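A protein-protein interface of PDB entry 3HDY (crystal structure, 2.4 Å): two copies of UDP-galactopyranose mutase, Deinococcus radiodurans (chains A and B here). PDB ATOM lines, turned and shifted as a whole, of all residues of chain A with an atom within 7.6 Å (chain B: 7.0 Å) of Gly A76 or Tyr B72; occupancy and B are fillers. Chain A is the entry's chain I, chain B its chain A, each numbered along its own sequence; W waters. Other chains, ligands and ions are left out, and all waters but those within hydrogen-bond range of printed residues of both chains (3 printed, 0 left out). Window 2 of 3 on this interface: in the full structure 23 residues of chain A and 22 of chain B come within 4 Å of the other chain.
The side-chain carboxylate of Asp A74 is in salt-bridge range of the guanidinium group of Arg B224, 2.9 Å away.
The side-chain carboxylate (OD1) of Asp B74 lies within salt-bridge range of the guanidinium group (NH2) of Arg A224, 2.7 Å away.
The side-chain carboxylate of Asp B73 is in hydrogen-bond range of the backbone NH of Ala B75 (3.1 Å).
OD1 of Asp B73 is in hydrogen-bond range of N of Gly B76, at 3.0 Å.
The side-chain amide nitrogen (NE2) of Gln A315 sits at hydrogen-bond distance from the backbone carbonyl oxygen (O) of Gly A76.
The side-chain carboxylate of Asp A73 lies within hydrogen-bond range of the backbone NH of Gly A76, at 2.9 Å.
The side-chain carboxylate (OD1) of Asp B73 is in hydrogen-bond range of the backbone NH (N) of Val B77 (2.7 Å).
Among the printed residues, pairs that only touch across the chains: Tyr A72 with Tyr B72, Tyr A72 with Asp B73, Asp A74 with His B220 and Gly A76 with Tyr B72.
Printed residues of chain B within 4 Å of Gly A76: Tyr B72 (3.99 Å).
Printed residues of chain A within 4 Å of Tyr B72: Tyr A72 and Gly A76.
Of the printed residues of chain A, His B220 touches Asp A74.
Of the printed residues of chain B, Asp A74 touches His B220 and Arg B224.
Of the 16 printed residues of chain A, 4 touch a printed residue of chain B.
Hydrophobic or aromatic side chains of chain A within 4 Å of the printed part of chain B: Tyr A72.
Printed residues of chain B that touch a printed residue of chain A: Tyr B72, Asp B73, Asp B74, His B220 and Arg B224.
Among the printed residues, Asp or Glu carboxylates within 4 Å of a Lys or Arg side-chain nitrogen of the other chain: Asp A74 with Arg B224 and Arg A224 with Asp B74.
Tyr B72 touches its own counterpart, Tyr A72.
Tyr A72 touches Asp B73, but with the chains exchanged Asp A73 does not touch Tyr B72 (4.03 Å).
Asp A74 touches Arg B224, and with the chains exchanged Arg A224 touches Asp B74.
Gly A76 touches Tyr B72, but with the chains exchanged Tyr A72 does not touch Gly B76 (4.02 Å).
12 positions are printed for both chains.
Of the 6 pairs that touch across the chains among the printed residues, 3 have their exchanged pair printed and touching as well.
Water W3 lies within hydrogen-bond range of O of Gly B76 (2.6 Å), O of Gly A76 (2.8 Å) and NE2 of Gln B315 (3.3 Å).
Water W1 bridges ND1 of His B220 (3.0 Å) and O of Asp A74 (3.4 Å).
Water W2 bridges NH2 of Arg A224 and OD1 of Asp B74.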
ATOM      1  N   CYS A  71     -20.288   8.101  20.607  1.00  0.00           N
ATOM      2  CA  CYS A  71     -19.187   7.157  20.714  1.00  0.00           C
ATOM      3  C   CYS A  71     -17.865   7.907  20.649  1.00  0.00           C
ATOM      4  O   CYS A  71     -17.836   9.075  20.259  1.00  0.00           O
ATOM      5  CB  CYS A  71     -19.262   6.122  19.588  1.00  0.00           C
ATOM      6  SG  CYS A  71     -19.134   6.820  17.917  1.00  0.00           S
ATOM      7  N   TYR A  72     -16.785   7.236  21.046  1.00  0.00           N
ATOM      8  CA  TYR A  72     -15.438   7.797  20.974  1.00  0.00           C
ATOM      9  C   TYR A  72     -14.844   7.573  19.590  1.00  0.00           C
ATOM     10  O   TYR A  72     -14.907   6.463  19.059  1.00  0.00           O
ATOM     11  CB  TYR A  72     -14.524   7.154  22.022  1.00  0.00           C
ATOM     12  CG  TYR A  72     -14.863   7.510  23.450  1.00  0.00           C
ATOM     13  CD1 TYR A  72     -14.155   8.491  24.129  1.00  0.00           C
ATOM     14  CD2 TYR A  72     -15.889   6.860  24.121  1.00  0.00           C
ATOM     15  CE1 TYR A  72     -14.461   8.816  25.435  1.00  0.00           C
ATOM     16  CE2 TYR A  72     -16.202   7.178  25.425  1.00  0.00           C
ATOM     17  CZ  TYR A  72     -15.487   8.156  26.079  1.00  0.00           C
ATOM     18  OH  TYR A  72     -15.804   8.469  27.382  1.00  0.00           O
ATOM     19  N   ASP A  73     -14.260   8.624  19.019  1.00  0.00           N
ATOM     20  CA  ASP A  73     -13.612   8.539  17.715  1.00  0.00           C
ATOM     21  C   ASP A  73     -12.208   7.975  17.863  1.00  0.00           C
ATOM     22  O   ASP A  73     -11.777   7.657  18.971  1.00  0.00           O
ATOM     23  CB  ASP A  73     -13.558   9.916  17.045  1.00  0.00           C
ATOM     24  CG  ASP A  73     -12.799  10.948  17.874  1.00  0.00           C
ATOM     25  OD1 ASP A  73     -12.081  10.564  18.826  1.00  0.00           O
ATOM     26  OD2 ASP A  73     -12.918  12.151  17.562  1.00  0.00           O
ATOM     27  N   ASP A  74     -11.494   7.865  16.748  1.00  0.00           N
ATOM     28  CA  ASP A  74     -10.140   7.313  16.748  1.00  0.00           C
ATOM     29  C   ASP A  74      -9.194   8.054  17.696  1.00  0.00           C
ATOM     30  O   ASP A  74      -8.247   7.466  18.214  1.00  0.00           O
ATOM     31  CB  ASP A  74      -9.556   7.320  15.332  1.00  0.00           C
ATOM     32  CG  ASP A  74     -10.355   6.470  14.358  1.00  0.00           C
ATOM     33  OD1 ASP A  74     -11.149   5.617  14.810  1.00  0.00           O
ATOM     34  OD2 ASP A  74     -10.183   6.656  13.136  1.00  0.00           O
ATOM     35  N   ALA A  75      -9.444   9.342  17.917  1.00  0.00           N
ATOM     36  CA  ALA A  75      -8.594  10.143  18.792  1.00  0.00           C
ATOM     37  C   ALA A  75      -8.944   9.928  20.257  1.00  0.00           C
ATOM     38  O   ALA A  75      -8.179  10.297  21.152  1.00  0.00           O
ATOM     39  CB  ALA A  75      -8.695  11.617  18.434  1.00  0.00           C
ATOM     40  N   GLY A  76     -10.104   9.326  20.498  1.00  0.00           N
ATOM     41  CA  GLY A  76     -10.542   9.040  21.853  1.00  0.00           C
ATOM     42  C   GLY A  76     -11.390  10.154  22.429  1.00  0.00           C
ATOM     43  O   GLY A  76     -11.473  10.318  23.647  1.00  0.00           O
ATOM     44  N   VAL A  77     -12.018  10.924  21.547  1.00  0.00           N
ATOM     45  CA  VAL A  77     -12.897  12.010  21.961  1.00  0.00           C
ATOM     46  C   VAL A  77     -14.353  11.586  21.808  1.00  0.00           C
ATOM     47  O   VAL A  77     -14.711  10.921  20.836  1.00  0.00           O
ATOM     48  CB  VAL A  77     -12.642  13.280  21.130  1.00  0.00           C
ATOM     49  CG1 VAL A  77     -13.540  14.412  21.589  1.00  0.00           C
ATOM     50  CG2 VAL A  77     -11.184  13.682  21.224  1.00  0.00           C
ATOM     51  N   LEU A  78     -15.183  11.965  22.774  1.00  0.00           N
ATOM     52  CA  LEU A  78     -16.604  11.624  22.746  1.00  0.00           C
ATOM     53  C   LEU A  78     -17.316  12.546  21.767  1.00  0.00           C
ATOM     54  O   LEU A  78     -17.203  13.768  21.868  1.00  0.00           O
ATOM     55  CB  LEU A  78     -17.210  11.756  24.148  1.00  0.00           C
ATOM     56  CG  LEU A  78     -18.658  11.311  24.386  1.00  0.00           C
ATOM     57  CD1 LEU A  78     -18.883   9.864  23.965  1.00  0.00           C
ATOM     58  CD2 LEU A  78     -19.029  11.507  25.847  1.00  0.00           C
ATOM     59  N   ILE A  79     -18.044  11.962  20.819  1.00  0.00           N
ATOM     60  CA  ILE A  79     -18.713  12.741  19.779  1.00  0.00           C
ATOM     61  C   ILE A  79     -20.124  12.245  19.461  1.00  0.00           C
ATOM     62  O   ILE A  79     -20.487  11.115  19.782  1.00  0.00           O
ATOM     63  CB  ILE A  79     -17.918  12.710  18.464  1.00  0.00           C
ATOM     64  CG1 ILE A  79     -17.933  11.296  17.876  1.00  0.00           C
ATOM     65  CG2 ILE A  79     -16.491  13.190  18.686  1.00  0.00           C
ATOM     66  CD1 ILE A  79     -17.641  11.245  16.391  1.00  0.00           C
ATOM     67  N   ARG A 224     -24.471   5.321  26.730  1.00  0.00           N
ATOM     68  CA  ARG A 224     -24.399   4.703  28.051  1.00  0.00           C
ATOM     69  C   ARG A 224     -25.762   4.708  28.727  1.00  0.00           C
ATOM     70  O   ARG A 224     -26.125   3.760  29.420  1.00  0.00           O
ATOM     71  CB  ARG A 224     -23.367   5.428  28.925  1.00  0.00           C
ATOM     72  CG  ARG A 224     -21.919   5.150  28.539  1.00  0.00           C
ATOM     73  CD  ARG A 224     -21.437   3.806  29.076  1.00  0.00           C
ATOM     74  NE  ARG A 224     -21.500   3.766  30.531  1.00  0.00           N
ATOM     75  CZ  ARG A 224     -20.520   4.163  31.338  1.00  0.00           C
ATOM     76  NH1 ARG A 224     -19.383   4.625  30.835  1.00  0.00           N
ATOM     77  NH2 ARG A 224     -20.677   4.092  32.652  1.00  0.00           N
ATOM     78  N   THR A 283     -10.712  16.129  13.721  1.00  0.00           N
ATOM     79  CA  THR A 283      -9.986  16.193  14.979  1.00  0.00           C
ATOM     80  C   THR A 283      -8.780  17.114  14.828  1.00  0.00           C
ATOM     81  O   THR A 283      -7.964  16.943  13.923  1.00  0.00           O
ATOM     82  CB  THR A 283      -9.516  14.801  15.424  1.00  0.00           C
ATOM     83  OG1 THR A 283     -10.654  13.945  15.576  1.00  0.00           O
ATOM     84  CG2 THR A 283      -8.765  14.884  16.750  1.00  0.00           C
ATOM     85  N   GLN A 315     -15.554  16.840  28.464  1.00  0.00           N
ATOM     86  CA  GLN A 315     -14.424  15.919  28.450  1.00  0.00           C
ATOM     87  C   GLN A 315     -13.097  16.667  28.382  1.00  0.00           C
ATOM     88  O   GLN A 315     -12.983  17.690  27.708  1.00  0.00           O
ATOM     89  CB  GLN A 315     -14.525  14.947  27.274  1.00  0.00           C
ATOM     90  CG  GLN A 315     -13.378  13.946  27.196  1.00  0.00           C
ATOM     91  CD  GLN A 315     -13.335  13.213  25.871  1.00  0.00           C
ATOM     92  OE1 GLN A 315     -14.084  13.535  24.946  1.00  0.00           O
ATOM     93  NE2 GLN A 315     -12.455  12.223  25.769  1.00  0.00           N
ATOM     94  N   ARG A 316     -12.099  16.144  29.083  1.00  0.00           N
ATOM     95  CA  ARG A 316     -10.755  16.700  29.047  1.00  0.00           C
ATOM     96  C   ARG A 316      -9.893  15.898  28.078  1.00  0.00           C
ATOM     97  O   ARG A 316      -9.845  14.671  28.146  1.00  0.00           O
ATOM     98  CB  ARG A 316     -10.144  16.675  30.444  1.00  0.00           C
ATOM     99  CG  ARG A 316      -8.723  17.179  30.515  1.00  0.00           C
ATOM    100  CD  ARG A 316      -8.272  17.248  31.954  1.00  0.00           C
ATOM    101  NE  ARG A 316      -6.837  17.474  32.066  1.00  0.00           N
ATOM    102  CZ  ARG A 316      -6.170  17.413  33.213  1.00  0.00           C
ATOM    103  NH1 ARG A 316      -6.815  17.132  34.338  1.00  0.00           N
ATOM    104  NH2 ARG A 316      -4.861  17.630  33.233  1.00  0.00           N
ATOM    105  N   HIS A 317      -9.214  16.593  27.174  1.00  0.00           N
ATOM    106  CA  HIS A 317      -8.438  15.930  26.136  1.00  0.00           C
ATOM    107  C   HIS A 317      -7.393  16.893  25.598  1.00  0.00           C
ATOM    108  O   HIS A 317      -7.608  18.103  25.599  1.00  0.00           O
ATOM    109  CB  HIS A 317      -9.361  15.485  25.004  1.00  0.00           C
ATOM    110  CG  HIS A 317      -8.840  14.325  24.217  1.00  0.00           C
ATOM    111  ND1 HIS A 317      -7.938  14.469  23.185  1.00  0.00           N
ATOM    112  CD2 HIS A 317      -9.102  12.998  24.305  1.00  0.00           C
ATOM    113  CE1 HIS A 317      -7.666  13.282  22.672  1.00  0.00           C
ATOM    114  NE2 HIS A 317      -8.360  12.372  23.334  1.00  0.00           N
ATOM    115  N   GLN A 319      -6.442  16.841  22.528  1.00  0.00           N
ATOM    116  CA  GLN A 319      -6.962  17.184  21.213  1.00  0.00           C
ATOM    117  C   GLN A 319      -8.434  17.584  21.311  1.00  0.00           C
ATOM    118  O   GLN A 319      -9.004  17.631  22.404  1.00  0.00           O
ATOM    119  CB  GLN A 319      -6.775  16.021  20.237  1.00  0.00           C
ATOM    120  CG  GLN A 319      -5.316  15.739  19.897  1.00  0.00           C
ATOM    121  CD  GLN A 319      -5.152  14.655  18.845  1.00  0.00           C
ATOM    122  OE1 GLN A 319      -5.707  13.562  18.968  1.00  0.00           O
ATOM    123  NE2 GLN A 319      -4.379  14.952  17.808  1.00  0.00           N
ATOM    124  N   SER A 321     -12.380  17.405  18.910  1.00  0.00           N
ATOM    125  CA  SER A 321     -13.101  16.964  17.729  1.00  0.00           C
ATOM    126  C   SER A 321     -14.270  17.889  17.430  1.00  0.00           C
ATOM    127  O   SER A 321     -14.990  18.316  18.335  1.00  0.00           O
ATOM    128  CB  SER A 321     -13.597  15.528  17.908  1.00  0.00           C
ATOM    129  OG  SER A 321     -12.517  14.612  17.906  1.00  0.00           O
ATOM    130  N   TYR B  69     -14.069  -8.239  24.124  1.00  0.00           N
ATOM    131  CA  TYR B  69     -14.758  -6.957  24.065  1.00  0.00           C
ATOM    132  C   TYR B  69     -13.945  -5.887  24.782  1.00  0.00           C
ATOM    133  O   TYR B  69     -13.345  -6.143  25.827  1.00  0.00           O
ATOM    134  CB  TYR B  69     -16.146  -7.086  24.692  1.00  0.00           C
ATOM    135  CG  TYR B  69     -16.902  -5.789  24.876  1.00  0.00           C
ATOM    136  CD1 TYR B  69     -17.398  -5.087  23.785  1.00  0.00           C
ATOM    137  CD2 TYR B  69     -17.151  -5.285  26.144  1.00  0.00           C
ATOM    138  CE1 TYR B  69     -18.104  -3.909  23.950  1.00  0.00           C
ATOM    139  CE2 TYR B  69     -17.853  -4.105  26.321  1.00  0.00           C
ATOM    140  CZ  TYR B  69     -18.330  -3.424  25.220  1.00  0.00           C
ATOM    141  OH  TYR B  69     -19.033  -2.253  25.390  1.00  0.00           O
ATOM    142  N   ASP B  70     -13.910  -4.690  24.207  1.00  0.00           N
ATOM    143  CA  ASP B  70     -13.251  -3.565  24.857  1.00  0.00           C
ATOM    144  C   ASP B  70     -14.072  -2.288  24.739  1.00  0.00           C
ATOM    145  O   ASP B  70     -14.833  -2.107  23.790  1.00  0.00           O
ATOM    146  CB  ASP B  70     -11.827  -3.359  24.324  1.00  0.00           C
ATOM    147  CG  ASP B  70     -11.786  -3.026  22.839  1.00  0.00           C
ATOM    148  OD1 ASP B  70     -10.669  -2.920  22.298  1.00  0.00           O
ATOM    149  OD2 ASP B  70     -12.851  -2.869  22.209  1.00  0.00           O
ATOM    150  N   CYS B  71     -13.920  -1.407  25.717  1.00  0.00           N
ATOM    151  CA  CYS B  71     -14.700  -0.180  25.752  1.00  0.00           C
ATOM    152  C   CYS B  71     -13.977   0.895  26.554  1.00  0.00           C
ATOM    153  O   CYS B  71     -13.044   0.605  27.303  1.00  0.00           O
ATOM    154  CB  CYS B  71     -16.076  -0.446  26.371  1.00  0.00           C
ATOM    155  SG  CYS B  71     -16.024  -0.990  28.111  1.00  0.00           S
ATOM    156  N   TYR B  72     -14.411   2.138  26.391  1.00  0.00           N
ATOM    157  CA  TYR B  72     -13.910   3.222  27.218  1.00  0.00           C
ATOM    158  C   TYR B  72     -14.662   3.217  28.534  1.00  0.00           C
ATOM    159  O   TYR B  72     -15.849   2.888  28.577  1.00  0.00           O
ATOM    160  CB  TYR B  72     -14.079   4.566  26.506  1.00  0.00           C
ATOM    161  CG  TYR B  72     -13.214   4.702  25.275  1.00  0.00           C
ATOM    162  CD1 TYR B  72     -11.980   5.333  25.338  1.00  0.00           C
ATOM    163  CD2 TYR B  72     -13.624   4.185  24.054  1.00  0.00           C
ATOM    164  CE1 TYR B  72     -11.179   5.457  24.215  1.00  0.00           C
ATOM    165  CE2 TYR B  72     -12.829   4.303  22.925  1.00  0.00           C
ATOM    166  CZ  TYR B  72     -11.609   4.938  23.015  1.00  0.00           C
ATOM    167  OH  TYR B  72     -10.816   5.057  21.898  1.00  0.00           O
ATOM    168  N   ASP B  73     -13.969   3.558  29.613  1.00  0.00           N
ATOM    169  CA  ASP B  73     -14.601   3.628  30.925  1.00  0.00           C
ATOM    170  C   ASP B  73     -15.063   5.057  31.222  1.00  0.00           C
ATOM    171  O   ASP B  73     -15.077   5.907  30.335  1.00  0.00           O
ATOM    172  CB  ASP B  73     -13.649   3.115  32.010  1.00  0.00           C
ATOM    173  CG  ASP B  73     -12.330   3.874  32.043  1.00  0.00           C
ATOM    174  OD1 ASP B  73     -12.234   4.952  31.417  1.00  0.00           O
ATOM    175  OD2 ASP B  73     -11.388   3.392  32.702  1.00  0.00           O
ATOM    176  N   ASP B  74     -15.436   5.323  32.467  1.00  0.00           N
ATOM    177  CA  ASP B  74     -15.973   6.630  32.822  1.00  0.00           C
ATOM    178  C   ASP B  74     -14.916   7.717  32.713  1.00  0.00           C
ATOM    179  O   ASP B  74     -15.238   8.897  32.582  1.00  0.00           O
ATOM    180  CB  ASP B  74     -16.554   6.606  34.236  1.00  0.00           C
ATOM    181  CG  ASP B  74     -17.693   5.617  34.380  1.00  0.00           C
ATOM    182  OD1 ASP B  74     -18.439   5.425  33.398  1.00  0.00           O
ATOM    183  OD2 ASP B  74     -17.840   5.034  35.473  1.00  0.00           O
ATOM    184  N   ALA B  75     -13.651   7.311  32.758  1.00  0.00           N
ATOM    185  CA  ALA B  75     -12.542   8.257  32.724  1.00  0.00           C
ATOM    186  C   ALA B  75     -12.068   8.516  31.299  1.00  0.00           C
ATOM    187  O   ALA B  75     -11.273   9.422  31.057  1.00  0.00           O
ATOM    188  CB  ALA B  75     -11.393   7.758  33.581  1.00  0.00           C
ATOM    189  N   GLY B  76     -12.556   7.720  30.357  1.00  0.00           N
ATOM    190  CA  GLY B  76     -12.160   7.876  28.971  1.00  0.00           C
ATOM    191  C   GLY B  76     -10.949   7.031  28.637  1.00  0.00           C
ATOM    192  O   GLY B  76     -10.188   7.349  27.722  1.00  0.00           O
ATOM    193  N   VAL B  77     -10.769   5.950  29.389  1.00  0.00           N
ATOM    194  CA  VAL B  77      -9.672   5.021  29.159  1.00  0.00           C
ATOM    195  C   VAL B  77     -10.190   3.768  28.475  1.00  0.00           C
ATOM    196  O   VAL B  77     -11.116   3.118  28.965  1.00  0.00           O
ATOM    197  CB  VAL B  77      -8.988   4.620  30.483  1.00  0.00           C
ATOM    198  CG1 VAL B  77      -7.768   3.753  30.212  1.00  0.00           C
ATOM    199  CG2 VAL B  77      -8.610   5.854  31.281  1.00  0.00           C
ATOM    200  N   LEU B  78      -9.607   3.441  27.328  1.00  0.00           N
ATOM    201  CA  LEU B  78      -9.940   2.207  26.635  1.00  0.00           C
ATOM    202  C   LEU B  78      -9.462   1.029  27.486  1.00  0.00           C
ATOM    203  O   LEU B  78      -8.289   0.957  27.849  1.00  0.00           O
ATOM    204  CB  LEU B  78      -9.289   2.185  25.248  1.00  0.00           C
ATOM    205  CG  LEU B  78      -9.481   0.945  24.365  1.00  0.00           C
ATOM    206  CD1 LEU B  78     -10.959   0.647  24.127  1.00  0.00           C
ATOM    207  CD2 LEU B  78      -8.744   1.107  23.039  1.00  0.00           C
ATOM    208  N   ILE B  79     -10.373   0.117  27.816  1.00  0.00           N
ATOM    209  CA  ILE B  79     -10.039  -1.014  28.682  1.00  0.00           C
ATOM    210  C   ILE B  79     -10.672  -2.325  28.219  1.00  0.00           C
ATOM    211  O   ILE B  79     -11.564  -2.331  27.370  1.00  0.00           O
ATOM    212  CB  ILE B  79     -10.474  -0.764  30.139  1.00  0.00           C
ATOM    213  CG1 ILE B  79     -11.992  -0.875  30.267  1.00  0.00           C
ATOM    214  CG2 ILE B  79      -9.987   0.591  30.622  1.00  0.00           C
ATOM    215  CD1 ILE B  79     -12.490  -0.793  31.691  1.00  0.00           C
ATOM    216  N   HIS B 220      -7.698   0.407  17.011  1.00  0.00           N
ATOM    217  CA  HIS B 220      -8.763   1.128  17.702  1.00  0.00           C
ATOM    218  C   HIS B 220      -9.583   0.217  18.604  1.00  0.00           C
ATOM    219  O   HIS B 220     -10.726   0.527  18.943  1.00  0.00           O
ATOM    220  CB  HIS B 220      -9.666   1.846  16.702  1.00  0.00           C
ATOM    221  CG  HIS B 220      -8.937   2.806  15.819  1.00  0.00           C
ATOM    222  ND1 HIS B 220      -8.314   3.937  16.304  1.00  0.00           N
ATOM    223  CD2 HIS B 220      -8.725   2.804  14.482  1.00  0.00           C
ATOM    224  CE1 HIS B 220      -7.748   4.588  15.303  1.00  0.00           C
ATOM    225  NE2 HIS B 220      -7.985   3.923  14.187  1.00  0.00           N
ATOM    226  N   GLY B 221      -8.988  -0.905  18.991  1.00  0.00           N
ATOM    227  CA  GLY B 221      -9.635  -1.845  19.884  1.00  0.00           C
ATOM    228  C   GLY B 221     -10.263  -3.024  19.171  1.00  0.00           C
ATOM    229  O   GLY B 221     -10.409  -3.023  17.951  1.00  0.00           O
ATOM    230  N   ARG B 224     -14.131  -2.354  17.673  1.00  0.00           N
ATOM    231  CA  ARG B 224     -14.161  -1.723  16.365  1.00  0.00           C
ATOM    232  C   ARG B 224     -13.956  -2.770  15.287  1.00  0.00           C
ATOM    233  O   ARG B 224     -14.628  -2.759  14.259  1.00  0.00           O
ATOM    234  CB  ARG B 224     -13.074  -0.650  16.271  1.00  0.00           C
ATOM    235  CG  ARG B 224     -13.357   0.582  17.107  1.00  0.00           C
ATOM    236  CD  ARG B 224     -14.460   1.412  16.476  1.00  0.00           C
ATOM    237  NE  ARG B 224     -14.022   1.977  15.205  1.00  0.00           N
ATOM    238  CZ  ARG B 224     -13.351   3.119  15.091  1.00  0.00           C
ATOM    239  NH1 ARG B 224     -13.050   3.828  16.174  1.00  0.00           N
ATOM    240  NH2 ARG B 224     -12.985   3.554  13.894  1.00  0.00           N
ATOM    241  N   GLN B 315      -2.664   4.025  24.301  1.00  0.00           N
ATOM    242  CA  GLN B 315      -3.457   5.232  24.508  1.00  0.00           C
ATOM    243  C   GLN B 315      -2.732   6.288  25.343  1.00  0.00           C
ATOM    244  O   GLN B 315      -2.002   5.967  26.281  1.00  0.00           O
ATOM    245  CB  GLN B 315      -4.788   4.881  25.172  1.00  0.00           C
ATOM    246  CG  GLN B 315      -5.663   6.081  25.493  1.00  0.00           C
ATOM    247  CD  GLN B 315      -6.925   5.700  26.243  1.00  0.00           C
ATOM    248  OE1 GLN B 315      -7.019   4.613  26.818  1.00  0.00           O
ATOM    249  NE2 GLN B 315      -7.904   6.598  26.244  1.00  0.00           N
ATOM    250  N   HIS B 317      -3.238   9.476  27.905  1.00  0.00           N
ATOM    251  CA  HIS B 317      -4.251   9.922  28.855  1.00  0.00           C
ATOM    252  C   HIS B 317      -3.575  10.469  30.106  1.00  0.00           C
ATOM    253  O   HIS B 317      -2.478  10.034  30.463  1.00  0.00           O
ATOM    254  CB  HIS B 317      -5.164   8.752  29.226  1.00  0.00           C
ATOM    255  CG  HIS B 317      -6.498   9.170  29.762  1.00  0.00           C
ATOM    256  ND1 HIS B 317      -6.656   9.745  31.005  1.00  0.00           N
ATOM    257  CD2 HIS B 317      -7.739   9.086  29.227  1.00  0.00           C
ATOM    258  CE1 HIS B 317      -7.935  10.000  31.210  1.00  0.00           C
ATOM    259  NE2 HIS B 317      -8.614   9.610  30.147  1.00  0.00           N
HETATM  260  O   HOH W   1      -8.333   4.246  19.304  1.00  0.00           O
HETATM  261  O   HOH W   2     -18.525   1.995  33.906  1.00  0.00           O
HETATM  262  O   HOH W   3     -10.121   9.052  25.710  1.00  0.00           O
